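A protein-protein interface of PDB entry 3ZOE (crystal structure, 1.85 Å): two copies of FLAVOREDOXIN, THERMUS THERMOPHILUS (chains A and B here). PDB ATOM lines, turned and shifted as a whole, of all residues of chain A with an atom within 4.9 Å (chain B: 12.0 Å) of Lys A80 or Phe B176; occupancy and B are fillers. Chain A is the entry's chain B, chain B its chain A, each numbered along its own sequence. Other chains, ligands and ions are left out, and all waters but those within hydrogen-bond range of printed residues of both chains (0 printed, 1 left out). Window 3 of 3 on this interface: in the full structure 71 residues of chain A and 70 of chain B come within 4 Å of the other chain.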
ATOM      1  N   PRO A  76       7.823 -14.307  26.542  1.00  0.00           N
ATOM      2  CA  PRO A  76       8.343 -14.724  25.265  1.00  0.00           C
ATOM      3  C   PRO A  76       9.632 -15.523  25.405  1.00  0.00           C
ATOM      4  O   PRO A  76      10.401 -15.347  26.387  1.00  0.00           O
ATOM      5  CB  PRO A  76       8.595 -13.390  24.529  1.00  0.00           C
ATOM      6  CG  PRO A  76       8.896 -12.424  25.580  1.00  0.00           C
ATOM      7  CD  PRO A  76       7.986 -12.852  26.747  1.00  0.00           C
ATOM      8  N   PHE A  77       9.869 -16.373  24.421  1.00  0.00           N
ATOM      9  CA  PHE A  77      11.055 -17.230  24.352  1.00  0.00           C
ATOM     10  C   PHE A  77      12.323 -16.438  24.776  1.00  0.00           C
ATOM     11  O   PHE A  77      13.202 -16.980  25.397  1.00  0.00           O
ATOM     12  CB  PHE A  77      11.215 -17.785  22.920  1.00  0.00           C
ATOM     13  CG  PHE A  77      11.725 -16.756  21.937  1.00  0.00           C
ATOM     14  CD1 PHE A  77      13.099 -16.542  21.776  1.00  0.00           C
ATOM     15  CD2 PHE A  77      10.838 -15.959  21.217  1.00  0.00           C
ATOM     16  CE1 PHE A  77      13.569 -15.556  20.913  1.00  0.00           C
ATOM     17  CE2 PHE A  77      11.308 -14.974  20.361  1.00  0.00           C
ATOM     18  CZ  PHE A  77      12.664 -14.779  20.226  1.00  0.00           C
ATOM     19  N   GLY A  78      12.379 -15.146  24.453  1.00  0.00           N
ATOM     20  CA  GLY A  78      13.586 -14.310  24.675  1.00  0.00           C
ATOM     21  C   GLY A  78      13.943 -14.210  26.135  1.00  0.00           C
ATOM     22  O   GLY A  78      15.098 -13.947  26.469  1.00  0.00           O
ATOM     23  N   GLN A  79      12.974 -14.509  27.022  1.00  0.00           N
ATOM     24  CA  GLN A  79      13.261 -14.473  28.434  1.00  0.00           C
ATOM     25  C   GLN A  79      13.487 -15.830  29.085  1.00  0.00           C
ATOM     26  O   GLN A  79      13.347 -15.934  30.300  1.00  0.00           O
ATOM     27  CB  GLN A  79      12.149 -13.697  29.150  1.00  0.00           C
ATOM     28  CG  GLN A  79      12.119 -12.247  28.756  1.00  0.00           C
ATOM     29  CD  GLN A  79      11.098 -11.477  29.536  1.00  0.00           C
ATOM     30  OE1 GLN A  79       9.893 -11.610  29.310  1.00  0.00           O
ATOM     31  NE2 GLN A  79      11.566 -10.635  30.429  1.00  0.00           N
ATOM     32  N   LYS A  80      13.876 -16.853  28.326  1.00  0.00           N
ATOM     33  CA  LYS A  80      14.104 -18.163  28.921  1.00  0.00           C
ATOM     34  C   LYS A  80      15.088 -18.157  30.076  1.00  0.00           C
ATOM     35  O   LYS A  80      14.839 -18.876  31.052  1.00  0.00           O
ATOM     36  CB  LYS A  80      14.511 -19.246  27.904  1.00  0.00           C
ATOM     37  CG  LYS A  80      15.846 -19.052  27.252  1.00  0.00           C
ATOM     38  CD  LYS A  80      16.259 -20.263  26.404  1.00  0.00           C
ATOM     39  CE  LYS A  80      17.726 -20.149  26.035  1.00  0.00           C
ATOM     40  NZ  LYS A  80      18.622 -20.245  27.219  1.00  0.00           N
ATOM     41  N   ASP A  81      16.173 -17.356  29.966  1.00  0.00           N
ATOM     42  CA  ASP A  81      17.258 -17.346  30.963  1.00  0.00           C
ATOM     43  C   ASP A  81      16.788 -16.760  32.289  1.00  0.00           C
ATOM     44  O   ASP A  81      17.093 -17.289  33.321  1.00  0.00           O
ATOM     45  CB  ASP A  81      18.505 -16.564  30.498  1.00  0.00           C
ATOM     46  CG  ASP A  81      19.264 -17.231  29.352  1.00  0.00           C
ATOM     47  OD1 ASP A  81      19.214 -18.450  29.155  1.00  0.00           O
ATOM     48  OD2 ASP A  81      19.994 -16.521  28.641  1.00  0.00           O
ATOM     49  N   LEU A  82      16.031 -15.667  32.232  1.00  0.00           N
ATOM     50  CA  LEU A  82      15.432 -15.029  33.423  1.00  0.00           C
ATOM     51  C   LEU A  82      14.402 -15.955  34.093  1.00  0.00           C
ATOM     52  O   LEU A  82      14.408 -16.113  35.315  1.00  0.00           O
ATOM     53  CB  LEU A  82      14.747 -13.703  33.064  1.00  0.00           C
ATOM     54  CG  LEU A  82      13.964 -12.975  34.168  1.00  0.00           C
ATOM     55  CD1 LEU A  82      14.833 -12.749  35.396  1.00  0.00           C
ATOM     56  CD2 LEU A  82      13.329 -11.642  33.742  1.00  0.00           C
ATOM     57  N   VAL A  83      13.510 -16.532  33.294  1.00  0.00           N
ATOM     58  CA  VAL A  83      12.518 -17.444  33.792  1.00  0.00           C
ATOM     59  C   VAL A  83      13.195 -18.623  34.507  1.00  0.00           C
ATOM     60  O   VAL A  83      12.793 -18.974  35.628  1.00  0.00           O
ATOM     61  CB  VAL A  83      11.559 -17.930  32.699  1.00  0.00           C
ATOM     62  CG1 VAL A  83      10.670 -19.037  33.229  1.00  0.00           C
ATOM     63  CG2 VAL A  83      10.694 -16.796  32.181  1.00  0.00           C
ATOM     64  N   HIS A  84      14.231 -19.190  33.898  1.00  0.00           N
ATOM     65  CA  HIS A  84      14.911 -20.327  34.482  1.00  0.00           C
ATOM     66  C   HIS A  84      15.577 -19.930  35.816  1.00  0.00           C
ATOM     67  O   HIS A  84      15.418 -20.634  36.878  1.00  0.00           O
ATOM     68  CB  HIS A  84      15.934 -20.938  33.540  1.00  0.00           C
ATOM     69  CG  HIS A  84      16.572 -22.154  34.112  1.00  0.00           C
ATOM     70  ND1 HIS A  84      15.850 -23.263  34.456  1.00  0.00           N
ATOM     71  CD2 HIS A  84      17.848 -22.389  34.508  1.00  0.00           C
ATOM     72  CE1 HIS A  84      16.654 -24.152  35.019  1.00  0.00           C
ATOM     73  NE2 HIS A  84      17.871 -23.637  35.069  1.00  0.00           N
ATOM     74  N   LEU A 160       7.280 -18.996  25.409  1.00  0.00           N
ATOM     75  CA  LEU A 160       8.275 -19.876  26.029  1.00  0.00           C
ATOM     76  C   LEU A 160       7.592 -21.183  26.414  1.00  0.00           C
ATOM     77  O   LEU A 160       6.501 -21.147  26.984  1.00  0.00           O
ATOM     78  CB  LEU A 160       8.936 -19.177  27.230  1.00  0.00           C
ATOM     79  CG  LEU A 160       9.947 -19.971  28.084  1.00  0.00           C
ATOM     80  CD1 LEU A 160      11.237 -20.187  27.312  1.00  0.00           C
ATOM     81  CD2 LEU A 160      10.193 -19.312  29.466  1.00  0.00           C
ATOM     82  N   GLY A 166      15.112 -28.560  33.131  1.00  0.00           N
ATOM     83  CA  GLY A 166      15.953 -27.511  32.602  1.00  0.00           C
ATOM     84  C   GLY A 166      15.952 -27.320  31.098  1.00  0.00           C
ATOM     85  O   GLY A 166      16.866 -26.682  30.579  1.00  0.00           O
ATOM     86  N   LEU A 167      14.934 -27.829  30.387  1.00  0.00           N
ATOM     87  CA  LEU A 167      14.948 -27.752  28.939  1.00  0.00           C
ATOM     88  C   LEU A 167      13.760 -26.936  28.453  1.00  0.00           C
ATOM     89  O   LEU A 167      12.615 -27.213  28.832  1.00  0.00           O
ATOM     90  CB  LEU A 167      14.896 -29.150  28.311  1.00  0.00           C
ATOM     91  CG  LEU A 167      14.993 -29.032  26.800  1.00  0.00           C
ATOM     92  CD1 LEU A 167      16.468 -28.782  26.417  1.00  0.00           C
ATOM     93  CD2 LEU A 167      14.448 -30.267  26.098  1.00  0.00           C
ATOM     94  N   TYR A 168      14.053 -25.981  27.582  1.00  0.00           N
ATOM     95  CA  TYR A 168      13.113 -24.986  27.100  1.00  0.00           C
ATOM     96  C   TYR A 168      13.043 -25.004  25.583  1.00  0.00           C
ATOM     97  O   TYR A 168      13.990 -25.415  24.900  1.00  0.00           O
ATOM     98  CB  TYR A 168      13.575 -23.602  27.539  1.00  0.00           C
ATOM     99  CG  TYR A 168      13.487 -23.389  29.018  1.00  0.00           C
ATOM    100  CD1 TYR A 168      14.513 -23.797  29.867  1.00  0.00           C
ATOM    101  CD2 TYR A 168      12.339 -22.834  29.592  1.00  0.00           C
ATOM    102  CE1 TYR A 168      14.392 -23.638  31.252  1.00  0.00           C
ATOM    103  CE2 TYR A 168      12.249 -22.636  30.951  1.00  0.00           C
ATOM    104  CZ  TYR A 168      13.273 -23.052  31.784  1.00  0.00           C
ATOM    105  OH  TYR A 168      13.143 -22.866  33.150  1.00  0.00           O
ATOM    106  N   ASP B 149      12.081 -39.049  24.088  1.00  0.00           N
ATOM    107  CA  ASP B 149      13.498 -38.877  24.505  1.00  0.00           C
ATOM    108  C   ASP B 149      13.823 -39.621  25.841  1.00  0.00           C
ATOM    109  O   ASP B 149      12.987 -40.387  26.427  1.00  0.00           O
ATOM    110  CB  ASP B 149      13.854 -37.356  24.579  1.00  0.00           C
ATOM    111  CG  ASP B 149      13.278 -36.650  25.841  1.00  0.00           C
ATOM    112  OD1 ASP B 149      12.785 -37.339  26.780  1.00  0.00           O
ATOM    113  OD2 ASP B 149      13.349 -35.401  25.892  1.00  0.00           O
ATOM    114  N   ARG B 153       9.556 -37.607  27.572  1.00  0.00           N
ATOM    115  CA  ARG B 153       8.933 -36.516  26.814  1.00  0.00           C
ATOM    116  C   ARG B 153       8.773 -36.870  25.332  1.00  0.00           C
ATOM    117  O   ARG B 153       9.569 -37.657  24.804  1.00  0.00           O
ATOM    118  CB  ARG B 153       9.800 -35.272  26.879  1.00  0.00           C
ATOM    119  CG  ARG B 153      10.536 -35.034  28.199  1.00  0.00           C
ATOM    120  CD  ARG B 153      11.447 -33.841  27.970  1.00  0.00           C
ATOM    121  NE  ARG B 153      12.151 -33.376  29.158  1.00  0.00           N
ATOM    122  CZ  ARG B 153      13.468 -33.216  29.256  1.00  0.00           C
ATOM    123  NH1 ARG B 153      14.297 -33.503  28.253  1.00  0.00           N
ATOM    124  NH2 ARG B 153      13.964 -32.773  30.389  1.00  0.00           N
ATOM    125  N   PRO B 154       7.795 -36.245  24.637  1.00  0.00           N
ATOM    126  CA  PRO B 154       7.861 -36.417  23.165  1.00  0.00           C
ATOM    127  C   PRO B 154       9.198 -35.893  22.656  1.00  0.00           C
ATOM    128  O   PRO B 154       9.658 -34.853  23.104  1.00  0.00           O
ATOM    129  CB  PRO B 154       6.705 -35.560  22.629  1.00  0.00           C
ATOM    130  CG  PRO B 154       6.305 -34.627  23.776  1.00  0.00           C
ATOM    131  CD  PRO B 154       6.802 -35.229  25.055  1.00  0.00           C
ATOM    132  N   LYS B 155       9.796 -36.622  21.725  1.00  0.00           N
ATOM    133  CA  LYS B 155      10.919 -36.119  20.939  1.00  0.00           C
ATOM    134  C   LYS B 155      10.637 -34.805  20.208  1.00  0.00           C
ATOM    135  O   LYS B 155       9.478 -34.495  19.866  1.00  0.00           O
ATOM    136  CB  LYS B 155      11.317 -37.180  19.914  1.00  0.00           C
ATOM    137  CG  LYS B 155      12.085 -38.341  20.504  1.00  0.00           C
ATOM    138  CD  LYS B 155      12.556 -39.287  19.402  1.00  0.00           C
ATOM    139  CE  LYS B 155      13.509 -40.342  19.945  1.00  0.00           C
ATOM    140  NZ  LYS B 155      13.373 -41.622  19.153  1.00  0.00           N
ATOM    141  N   PRO B 156      11.710 -34.021  19.937  1.00  0.00           N
ATOM    142  CA  PRO B 156      11.571 -32.673  19.396  1.00  0.00           C
ATOM    143  C   PRO B 156      10.508 -32.523  18.317  1.00  0.00           C
ATOM    144  O   PRO B 156      10.452 -33.330  17.364  1.00  0.00           O
ATOM    145  CB  PRO B 156      12.974 -32.379  18.793  1.00  0.00           C
ATOM    146  CG  PRO B 156      13.897 -33.478  19.293  1.00  0.00           C
ATOM    147  CD  PRO B 156      13.117 -34.317  20.277  1.00  0.00           C
ATOM    148  N   GLY B 157       9.665 -31.506  18.455  1.00  0.00           N
ATOM    149  CA  GLY B 157       8.638 -31.214  17.440  1.00  0.00           C
ATOM    150  C   GLY B 157       7.464 -32.167  17.286  1.00  0.00           C
ATOM    151  O   GLY B 157       6.592 -31.927  16.452  1.00  0.00           O
ATOM    152  N   PRO B 171       5.849 -27.953  18.719  1.00  0.00           N
ATOM    153  CA  PRO B 171       7.052 -27.203  19.129  1.00  0.00           C
ATOM    154  C   PRO B 171       8.078 -27.102  18.003  1.00  0.00           C
ATOM    155  O   PRO B 171       8.122 -27.983  17.142  1.00  0.00           O
ATOM    156  CB  PRO B 171       7.633 -28.047  20.271  1.00  0.00           C
ATOM    157  CG  PRO B 171       6.586 -29.079  20.585  1.00  0.00           C
ATOM    158  CD  PRO B 171       5.783 -29.277  19.353  1.00  0.00           C
ATOM    159  N   ALA B 172       8.906 -26.059  18.044  1.00  0.00           N
ATOM    160  CA  ALA B 172      10.077 -25.983  17.189  1.00  0.00           C
ATOM    161  C   ALA B 172      11.084 -27.049  17.612  1.00  0.00           C
ATOM    162  O   ALA B 172      11.164 -27.462  18.794  1.00  0.00           O
ATOM    163  CB  ALA B 172      10.715 -24.599  17.267  1.00  0.00           C
ATOM    164  N   GLU B 173      11.882 -27.481  16.640  1.00  0.00           N
ATOM    165  CA  GLU B 173      12.851 -28.527  16.890  1.00  0.00           C
ATOM    166  C   GLU B 173      13.934 -28.159  17.886  1.00  0.00           C
ATOM    167  O   GLU B 173      14.367 -29.016  18.650  1.00  0.00           O
ATOM    168  CB  GLU B 173      13.486 -28.955  15.576  1.00  0.00           C
ATOM    169  CG  GLU B 173      12.558 -29.829  14.754  1.00  0.00           C
ATOM    170  CD  GLU B 173      13.332 -30.854  13.980  1.00  0.00           C
ATOM    171  OE1 GLU B 173      14.487 -30.519  13.605  1.00  0.00           O
ATOM    172  OE2 GLU B 173      12.797 -31.970  13.775  1.00  0.00           O
ATOM    173  N   GLU B 174      14.313 -26.882  17.912  1.00  0.00           N
ATOM    174  CA  GLU B 174      15.474 -26.413  18.665  1.00  0.00           C
ATOM    175  C   GLU B 174      15.084 -26.216  20.122  1.00  0.00           C
ATOM    176  O   GLU B 174      14.084 -25.541  20.421  1.00  0.00           O
ATOM    177  CB  GLU B 174      16.008 -25.063  18.137  1.00  0.00           C
ATOM    178  CG  GLU B 174      15.880 -24.799  16.643  1.00  0.00           C
ATOM    179  CD  GLU B 174      16.957 -25.470  15.813  1.00  0.00           C
ATOM    180  OE1 GLU B 174      18.121 -25.023  15.892  1.00  0.00           O
ATOM    181  OE2 GLU B 174      16.634 -26.437  15.085  1.00  0.00           O
ATOM    182  N   THR B 175      15.875 -26.784  21.029  1.00  0.00           N
ATOM    183  CA  THR B 175      15.663 -26.577  22.461  1.00  0.00           C
ATOM    184  C   THR B 175      16.909 -25.953  23.099  1.00  0.00           C
ATOM    185  O   THR B 175      17.955 -25.799  22.433  1.00  0.00           O
ATOM    186  CB  THR B 175      15.275 -27.886  23.162  1.00  0.00           C
ATOM    187  OG1 THR B 175      16.236 -28.900  22.848  1.00  0.00           O
ATOM    188  CG2 THR B 175      13.884 -28.347  22.702  1.00  0.00           C
ATOM    189  N   PHE B 176      16.780 -25.557  24.373  1.00  0.00           N
ATOM    190  CA  PHE B 176      17.850 -24.871  25.091  1.00  0.00           C
ATOM    191  C   PHE B 176      17.833 -25.179  26.584  1.00  0.00           C
ATOM    192  O   PHE B 176      16.767 -25.208  27.223  1.00  0.00           O
ATOM    193  CB  PHE B 176      17.745 -23.359  24.895  1.00  0.00           C
ATOM    194  CG  PHE B 176      17.847 -22.930  23.463  1.00  0.00           C
ATOM    195  CD1 PHE B 176      19.086 -22.644  22.891  1.00  0.00           C
ATOM    196  CD2 PHE B 176      16.706 -22.830  22.673  1.00  0.00           C
ATOM    197  CE1 PHE B 176      19.179 -22.258  21.563  1.00  0.00           C
ATOM    198  CE2 PHE B 176      16.799 -22.457  21.334  1.00  0.00           C
ATOM    199  CZ  PHE B 176      18.032 -22.158  20.786  1.00  0.00           C
ATOM    200  N   ALA B 177      19.031 -25.389  27.127  1.00  0.00           N
ATOM    201  CA  ALA B 177      19.196 -25.840  28.500  1.00  0.00           C
ATOM    202  C   ALA B 177      20.362 -25.097  29.161  1.00  0.00           C
ATOM    203  O   ALA B 177      21.486 -25.610  29.174  1.00  0.00           O
ATOM    204  CB  ALA B 177      19.434 -27.340  28.524  1.00  0.00           C
ATOM    205  N   PRO B 178      20.093 -23.885  29.701  1.00  0.00           N
ATOM    206  CA  PRO B 178      21.116 -23.048  30.344  1.00  0.00           C
ATOM    207  C   PRO B 178      21.464 -23.507  31.764  1.00  0.00           C
ATOM    208  O   PRO B 178      22.613 -23.375  32.193  1.00  0.00           O
ATOM    209  CB  PRO B 178      20.464 -21.659  30.374  1.00  0.00           C
ATOM    210  CG  PRO B 178      19.000 -21.939  30.447  1.00  0.00           C
ATOM    211  CD  PRO B 178      18.780 -23.207  29.659  1.00  0.00           C
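The backbone NH of Phe B176 is in hydrogen-bond range of the backbone carbonyl oxygen of Tyr A168 (2.8 Å).
No position is printed for both chains.
Of the 14 printed residues of chain B, 5 touch a printed residue of chain A.
Of the 13 printed residues of chain A, 5 touch a printed residue of chain B.
Hydrophobic or aromatic side chains of chain A within 4 Å of the printed part of chain B: Leu A167 and Tyr A168.
Among the printed residues, no Asp or Glu carboxylate lies within 4 Å of a Lys or Arg side-chain nitrogen of the other chain.
A ring nitrogen (ND1) of His A84 is in hydrogen-bond range of the side-chain hydroxyl of Tyr A168.
OD1 of Asp A81 is in salt-bridge range of NZ of Lys A80, 2.7 Å away.
The guanidinium group (NH1) of Arg B153 is in salt-bridge range of the side-chain carboxylate (OD2) of Asp B149, at 3.2 Å.
Phe B176 touches Lys A80.
Lys A80 touches Pro B178.
Pro B178 touches Asp A81 (CB to OD1, 3.7 Å).
Gly A166 touches Phe B176 (O to O, 3.7 Å).
O of Gly A166 touches CA of Ala B177, at 3.2 Å.
Leu A167 touches Arg B153.
Thr B175 touches Leu A167.
Leu A167 touches Phe B176.
Leu A167 touches Ala B177 (CD1 to CB, 3.9 Å).
Tyr A168 touches Thr B175.
Of chain B, only Phe B176 and Pro B178 come within 4 Å of Lys A80.
Phe B176 touches just these residues of chain A: Lys A80, Gly A166, Leu A167 and Tyr A168.
No residue of chain B comes within 4 Å of Pro A76.
No residue of chain B comes within 4 Å of Gly A78.
No residue of chain B comes within 4 Å of Gln A79.
Of chain B, only Pro B178 (3.7 Å) comes within 4 Å of Asp A81.
No residue of chain B comes within 4 Å of Leu A82.
No residue of chain B comes within 4 Å of Val A83.
No residue of chain B comes within 4 Å of His A84.
Gly A166 touches just these residues of chain B: Phe B176 (3.7 Å) and Ala B177 (3.2 Å).
Leu A167 touches four residues of chain B.
Of the printed residues of chain A, Thr B175 touches Leu A167 and Tyr A168.
Of the printed residues of chain A, Ala B177 touches Gly A166 and Leu A167.
Gly B157 touches none of the printed residues of chain A.
Pro B171 touches none of the printed residues of chain A.
The nearest printed residue of chain A that does not touch Phe B176 is Asp A81 (6.7 Å).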
